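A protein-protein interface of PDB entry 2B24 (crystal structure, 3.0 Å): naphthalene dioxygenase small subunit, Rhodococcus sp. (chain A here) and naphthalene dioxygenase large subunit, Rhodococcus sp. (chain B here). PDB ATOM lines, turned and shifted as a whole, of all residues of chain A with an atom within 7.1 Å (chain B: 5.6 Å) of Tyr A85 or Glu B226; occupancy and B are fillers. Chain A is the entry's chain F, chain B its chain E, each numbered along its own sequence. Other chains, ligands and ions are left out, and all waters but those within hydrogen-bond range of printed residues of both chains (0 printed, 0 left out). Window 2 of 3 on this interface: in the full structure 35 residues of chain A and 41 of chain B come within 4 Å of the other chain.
The side-chain carboxylate of Asp B371 lies within hydrogen-bond range of the side-chain hydroxyl of Ser B223, at 3.3 Å. NE of Arg B222 is in salt-bridge range of OE1 of Glu B226 (2.7 Å).
Of chain B, only Arg B222 (3.5 Å), Ser B223 (3.0 Å) and Glu B226 (3.4 Å) come within 4 Å of Tyr A85. Of chain A, only Thr A83 and Tyr A85 come within 4 Å of Glu B226. Of the printed residues of chain B, Thr A83 touches Ser B223 (3.6 Å) and Glu B226 (2.8 Å). Printed residues of chain A within 4 Å of Arg B222: Tyr A85 (3.5 Å). Of the printed residues of chain A, Ser B223 touches Arg A80, Thr A83 and Tyr A85. Of the printed residues of chain A, Asp B371 touches Arg A80, Trp A87 and Ala A88. Of the printed residues of chain A, Met B219 touches Trp A87 (2.9 Å). The nearest printed residue of chain B that does not touch Arg A80 is Thr B220 (5.3 Å).
OE2 of Glu B226 lies within hydrogen-bond range of OG1 of Thr A83. OG of Ser B223 lies within hydrogen-bond range of O of Tyr A85 (3.0 Å). N of Ala A88 is in hydrogen-bond range of OD1 of Asp B371 (3.1 Å). NH1 of Arg A80 sits at hydrogen-bond distance from OG of Ser B223, 3.0 Å away. The indole nitrogen of Trp A87 sits close to the backbone carbonyl oxygen of Thr B220 (3.3 Å). The guanidinium group of Arg A80 lies within salt-bridge range of the side-chain carboxylate of Asp B371, at 2.9 Å. O of Met B219 is in hydrogen-bond range of NE1 of Trp A87 (2.9 Å).
Of the 10 printed residues of chain A, 5 touch a printed residue of chain B. Hydrophobic or aromatic side chains of chain B that line the printed part of chain A: Met B219, Met B224 and Leu B227. Among the printed residues, Asp or Glu carboxylates within 4 Å of a Lys or Arg side-chain nitrogen of the other chain: Arg A80 with Asp B371 (2.4 Å).
Met B224 touches Arg A80. CA of Arg A80 touches CD1 of Leu B227, 3.999 Å away. Thr A83 touches Ser B223. Tyr A85 touches Arg B222 (CD1 to CG, 3.5 Å). Tyr A85 touches Glu B226. Trp A87 touches Asp B371 (N to OD1, 3.8 Å).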
ATOM      1  N   ARG A  80      13.844  28.023  15.857  1.00  0.00           N
ATOM      2  CA  ARG A  80      15.109  27.780  16.523  1.00  0.00           C
ATOM      3  C   ARG A  80      16.216  27.494  15.514  1.00  0.00           C
ATOM      4  O   ARG A  80      17.335  27.981  15.639  1.00  0.00           O
ATOM      5  CB  ARG A  80      14.957  26.613  17.492  1.00  0.00           C
ATOM      6  CG  ARG A  80      15.938  26.628  18.629  1.00  0.00           C
ATOM      7  CD  ARG A  80      15.977  25.345  19.373  1.00  0.00           C
ATOM      8  NE  ARG A  80      16.798  24.338  18.718  1.00  0.00           N
ATOM      9  CZ  ARG A  80      18.090  24.162  18.949  1.00  0.00           C
ATOM     10  NH1 ARG A  80      18.721  24.958  19.802  1.00  0.00           N
ATOM     11  NH2 ARG A  80      18.750  23.192  18.324  1.00  0.00           N
ATOM     12  N   LEU A  81      15.880  26.696  14.510  1.00  0.00           N
ATOM     13  CA  LEU A  81      16.832  26.221  13.514  1.00  0.00           C
ATOM     14  C   LEU A  81      17.167  27.289  12.453  1.00  0.00           C
ATOM     15  O   LEU A  81      18.134  27.151  11.706  1.00  0.00           O
ATOM     16  CB  LEU A  81      16.283  24.959  12.844  1.00  0.00           C
ATOM     17  CG  LEU A  81      16.004  23.711  13.672  1.00  0.00           C
ATOM     18  CD1 LEU A  81      14.900  22.893  13.035  1.00  0.00           C
ATOM     19  CD2 LEU A  81      17.248  22.875  13.831  1.00  0.00           C
ATOM     20  N   GLU A  82      16.359  28.344  12.398  1.00  0.00           N
ATOM     21  CA  GLU A  82      16.570  29.468  11.490  1.00  0.00           C
ATOM     22  C   GLU A  82      17.498  30.493  12.084  1.00  0.00           C
ATOM     23  O   GLU A  82      18.005  31.345  11.387  1.00  0.00           O
ATOM     24  CB  GLU A  82      15.253  30.146  11.173  1.00  0.00           C
ATOM     25  CG  GLU A  82      14.358  29.326  10.276  1.00  0.00           C
ATOM     26  CD  GLU A  82      13.027  29.989  10.052  1.00  0.00           C
ATOM     27  OE1 GLU A  82      12.403  29.733   9.012  1.00  0.00           O
ATOM     28  OE2 GLU A  82      12.615  30.778  10.909  1.00  0.00           O
ATOM     29  N   THR A  83      17.678  30.414  13.390  1.00  0.00           N
ATOM     30  CA  THR A  83      18.673  31.183  14.115  1.00  0.00           C
ATOM     31  C   THR A  83      20.047  30.612  13.739  1.00  0.00           C
ATOM     32  O   THR A  83      20.134  29.503  13.195  1.00  0.00           O
ATOM     33  CB  THR A  83      18.355  31.097  15.646  1.00  0.00           C
ATOM     34  OG1 THR A  83      18.672  32.330  16.280  1.00  0.00           O
ATOM     35  CG2 THR A  83      19.236  30.115  16.356  1.00  0.00           C
ATOM     36  N   GLU A  84      21.118  31.359  13.986  1.00  0.00           N
ATOM     37  CA  GLU A  84      22.441  30.831  13.653  1.00  0.00           C
ATOM     38  C   GLU A  84      23.224  30.228  14.821  1.00  0.00           C
ATOM     39  O   GLU A  84      24.435  30.054  14.728  1.00  0.00           O
ATOM     40  CB  GLU A  84      23.298  31.848  12.892  1.00  0.00           C
ATOM     41  CG  GLU A  84      22.835  33.292  12.904  1.00  0.00           C
ATOM     42  CD  GLU A  84      23.786  34.170  12.113  1.00  0.00           C
ATOM     43  OE1 GLU A  84      23.650  34.205  10.878  1.00  0.00           O
ATOM     44  OE2 GLU A  84      24.683  34.801  12.723  1.00  0.00           O
ATOM     45  N   TYR A  85      22.519  29.893  15.904  1.00  0.00           N
ATOM     46  CA  TYR A  85      23.115  29.262  17.082  1.00  0.00           C
ATOM     47  C   TYR A  85      22.356  27.993  17.490  1.00  0.00           C
ATOM     48  O   TYR A  85      22.119  27.755  18.675  1.00  0.00           O
ATOM     49  CB  TYR A  85      23.193  30.250  18.262  1.00  0.00           C
ATOM     50  CG  TYR A  85      23.601  31.649  17.887  1.00  0.00           C
ATOM     51  CD1 TYR A  85      22.651  32.594  17.552  1.00  0.00           C
ATOM     52  CD2 TYR A  85      24.935  32.022  17.858  1.00  0.00           C
ATOM     53  CE1 TYR A  85      23.017  33.873  17.193  1.00  0.00           C
ATOM     54  CE2 TYR A  85      25.321  33.307  17.502  1.00  0.00           C
ATOM     55  CZ  TYR A  85      24.356  34.231  17.170  1.00  0.00           C
ATOM     56  OH  TYR A  85      24.692  35.520  16.807  1.00  0.00           O
ATOM     57  N   ALA A  86      21.984  27.186  16.499  1.00  0.00           N
ATOM     58  CA  ALA A  86      21.295  25.928  16.722  1.00  0.00           C
ATOM     59  C   ALA A  86      22.293  24.802  16.596  1.00  0.00           C
ATOM     60  O   ALA A  86      22.213  23.991  15.686  1.00  0.00           O
ATOM     61  CB  ALA A  86      20.166  25.752  15.744  1.00  0.00           C
ATOM     62  N   TRP A  87      23.215  24.756  17.553  1.00  0.00           N
ATOM     63  CA  TRP A  87      24.369  23.857  17.553  1.00  0.00           C
ATOM     64  C   TRP A  87      24.070  22.403  17.266  1.00  0.00           C
ATOM     65  O   TRP A  87      24.923  21.720  16.732  1.00  0.00           O
ATOM     66  CB  TRP A  87      25.136  23.960  18.874  1.00  0.00           C
ATOM     67  CG  TRP A  87      25.377  25.353  19.329  1.00  0.00           C
ATOM     68  CD1 TRP A  87      24.930  25.924  20.479  1.00  0.00           C
ATOM     69  CD2 TRP A  87      26.122  26.365  18.645  1.00  0.00           C
ATOM     70  NE1 TRP A  87      25.349  27.228  20.557  1.00  0.00           N
ATOM     71  CE2 TRP A  87      26.088  27.522  19.442  1.00  0.00           C
ATOM     72  CE3 TRP A  87      26.818  26.414  17.430  1.00  0.00           C
ATOM     73  CZ2 TRP A  87      26.717  28.711  19.064  1.00  0.00           C
ATOM     74  CZ3 TRP A  87      27.442  27.583  17.063  1.00  0.00           C
ATOM     75  CH2 TRP A  87      27.389  28.718  17.876  1.00  0.00           C
ATOM     76  N   ALA A  88      22.879  21.930  17.626  1.00  0.00           N
ATOM     77  CA  ALA A  88      22.532  20.521  17.474  1.00  0.00           C
ATOM     78  C   ALA A  88      22.376  20.177  16.022  1.00  0.00           C
ATOM     79  O   ALA A  88      22.432  19.005  15.657  1.00  0.00           O
ATOM     80  CB  ALA A  88      21.274  20.209  18.201  1.00  0.00           C
ATOM     81  N   ASP A  90      23.715  22.885  13.466  1.00  0.00           N
ATOM     82  CA  ASP A  90      24.261  24.036  12.723  1.00  0.00           C
ATOM     83  C   ASP A  90      25.454  23.818  11.819  1.00  0.00           C
ATOM     84  O   ASP A  90      25.678  24.645  10.903  1.00  0.00           O
ATOM     85  CB  ASP A  90      24.409  25.320  13.508  1.00  0.00           C
ATOM     86  CG  ASP A  90      24.220  26.544  12.625  1.00  0.00           C
ATOM     87  OD1 ASP A  90      24.816  26.574  11.535  1.00  0.00           O
ATOM     88  OD2 ASP A  90      23.481  27.515  12.916  1.00  0.00           O
ATOM     89  N   MET B 219      25.614  30.988  25.531  1.00  0.00           N
ATOM     90  CA  MET B 219      26.168  30.596  24.236  1.00  0.00           C
ATOM     91  C   MET B 219      25.482  29.379  23.642  1.00  0.00           C
ATOM     92  O   MET B 219      25.044  29.419  22.501  1.00  0.00           O
ATOM     93  CB  MET B 219      27.669  30.332  24.322  1.00  0.00           C
ATOM     94  CG  MET B 219      28.351  30.143  22.983  1.00  0.00           C
ATOM     95  SD  MET B 219      27.851  31.337  21.753  1.00  0.00           S
ATOM     96  CE  MET B 219      28.925  30.941  20.451  1.00  0.00           C
ATOM     97  N   THR B 220      25.405  28.295  24.408  1.00  0.00           N
ATOM     98  CA  THR B 220      24.828  27.062  23.893  1.00  0.00           C
ATOM     99  C   THR B 220      23.330  27.191  23.713  1.00  0.00           C
ATOM    100  O   THR B 220      22.810  26.780  22.684  1.00  0.00           O
ATOM    101  CB  THR B 220      25.282  25.783  24.694  1.00  0.00           C
ATOM    102  OG1 THR B 220      24.246  24.804  24.731  1.00  0.00           O
ATOM    103  CG2 THR B 220      25.485  26.074  26.111  1.00  0.00           C
ATOM    104  N   HIS B 221      22.651  27.809  24.677  1.00  0.00           N
ATOM    105  CA  HIS B 221      21.211  28.068  24.565  1.00  0.00           C
ATOM    106  C   HIS B 221      20.892  29.486  24.085  1.00  0.00           C
ATOM    107  O   HIS B 221      19.858  30.044  24.438  1.00  0.00           O
ATOM    108  CB  HIS B 221      20.498  27.750  25.879  1.00  0.00           C
ATOM    109  CG  HIS B 221      20.827  26.398  26.424  1.00  0.00           C
ATOM    110  ND1 HIS B 221      20.482  25.235  25.779  1.00  0.00           N
ATOM    111  CD2 HIS B 221      21.490  26.023  27.541  1.00  0.00           C
ATOM    112  CE1 HIS B 221      20.915  24.200  26.474  1.00  0.00           C
ATOM    113  NE2 HIS B 221      21.530  24.650  27.550  1.00  0.00           N
ATOM    114  N   ARG B 222      21.788  30.040  23.265  1.00  0.00           N
ATOM    115  CA  ARG B 222      21.623  31.339  22.595  1.00  0.00           C
ATOM    116  C   ARG B 222      20.443  31.354  21.642  1.00  0.00           C
ATOM    117  O   ARG B 222      19.777  32.368  21.507  1.00  0.00           O
ATOM    118  CB  ARG B 222      22.885  31.698  21.816  1.00  0.00           C
ATOM    119  CG  ARG B 222      22.784  32.949  20.998  1.00  0.00           C
ATOM    120  CD  ARG B 222      23.042  34.217  21.773  1.00  0.00           C
ATOM    121  NE  ARG B 222      22.520  35.386  21.071  1.00  0.00           N
ATOM    122  CZ  ARG B 222      22.209  36.532  21.644  1.00  0.00           C
ATOM    123  NH1 ARG B 222      22.365  36.701  22.947  1.00  0.00           N
ATOM    124  NH2 ARG B 222      21.746  37.520  20.907  1.00  0.00           N
ATOM    125  N   SER B 223      20.203  30.232  20.969  1.00  0.00           N
ATOM    126  CA  SER B 223      19.036  30.066  20.122  1.00  0.00           C
ATOM    127  C   SER B 223      17.801  30.449  20.896  1.00  0.00           C
ATOM    128  O   SER B 223      16.982  31.212  20.406  1.00  0.00           O
ATOM    129  CB  SER B 223      18.912  28.626  19.661  1.00  0.00           C
ATOM    130  OG  SER B 223      19.686  27.765  20.466  1.00  0.00           O
ATOM    131  N   MET B 224      17.702  29.932  22.124  1.00  0.00           N
ATOM    132  CA  MET B 224      16.556  30.117  23.013  1.00  0.00           C
ATOM    133  C   MET B 224      16.514  31.488  23.667  1.00  0.00           C
ATOM    134  O   MET B 224      15.472  31.897  24.140  1.00  0.00           O
ATOM    135  CB  MET B 224      16.565  29.051  24.104  1.00  0.00           C
ATOM    136  CG  MET B 224      16.361  27.641  23.637  1.00  0.00           C
ATOM    137  SD  MET B 224      15.031  27.551  22.555  1.00  0.00           S
ATOM    138  CE  MET B 224      13.944  26.474  23.357  1.00  0.00           C
ATOM    139  N   VAL B 225      17.656  32.176  23.721  1.00  0.00           N
ATOM    140  CA  VAL B 225      17.737  33.550  24.242  1.00  0.00           C
ATOM    141  C   VAL B 225      17.106  34.510  23.237  1.00  0.00           C
ATOM    142  O   VAL B 225      16.465  35.483  23.609  1.00  0.00           O
ATOM    143  CB  VAL B 225      19.205  33.979  24.549  1.00  0.00           C
ATOM    144  CG1 VAL B 225      19.322  35.485  24.649  1.00  0.00           C
ATOM    145  CG2 VAL B 225      19.730  33.330  25.830  1.00  0.00           C
ATOM    146  N   GLU B 226      17.289  34.191  21.958  1.00  0.00           N
ATOM    147  CA  GLU B 226      16.746  34.943  20.832  1.00  0.00           C
ATOM    148  C   GLU B 226      15.248  34.789  20.680  1.00  0.00           C
ATOM    149  O   GLU B 226      14.590  35.692  20.196  1.00  0.00           O
ATOM    150  CB  GLU B 226      17.412  34.482  19.544  1.00  0.00           C
ATOM    151  CG  GLU B 226      18.226  35.551  18.848  1.00  0.00           C
ATOM    152  CD  GLU B 226      19.589  35.054  18.423  1.00  0.00           C
ATOM    153  OE1 GLU B 226      20.468  34.975  19.292  1.00  0.00           O
ATOM    154  OE2 GLU B 226      19.779  34.756  17.227  1.00  0.00           O
ATOM    155  N   LEU B 227      14.708  33.643  21.078  1.00  0.00           N
ATOM    156  CA  LEU B 227      13.271  33.391  20.975  1.00  0.00           C
ATOM    157  C   LEU B 227      12.484  33.860  22.205  1.00  0.00           C
ATOM    158  O   LEU B 227      11.254  33.836  22.199  1.00  0.00           O
ATOM    159  CB  LEU B 227      12.988  31.904  20.702  1.00  0.00           C
ATOM    160  CG  LEU B 227      13.603  31.239  19.476  1.00  0.00           C
ATOM    161  CD1 LEU B 227      13.506  29.754  19.610  1.00  0.00           C
ATOM    162  CD2 LEU B 227      12.927  31.685  18.208  1.00  0.00           C
ATOM    163  N   GLY B 228      13.192  34.274  23.252  1.00  0.00           N
ATOM    164  CA  GLY B 228      12.571  34.705  24.487  1.00  0.00           C
ATOM    165  C   GLY B 228      12.191  33.572  25.414  1.00  0.00           C
ATOM    166  O   GLY B 228      11.295  33.725  26.242  1.00  0.00           O
ATOM    167  N   ASP B 371      20.829  20.732  22.293  1.00  0.00           N
ATOM    168  CA  ASP B 371      22.108  21.403  22.118  1.00  0.00           C
ATOM    169  C   ASP B 371      23.077  20.983  23.202  1.00  0.00           C
ATOM    170  O   ASP B 371      24.279  21.023  23.000  1.00  0.00           O
ATOM    171  CB  ASP B 371      21.930  22.917  22.206  1.00  0.00           C
ATOM    172  CG  ASP B 371      21.218  23.498  21.003  1.00  0.00           C
ATOM    173  OD1 ASP B 371      21.059  22.787  19.988  1.00  0.00           O
ATOM    174  OD2 ASP B 371      20.776  24.666  20.987  1.00  0.00           O
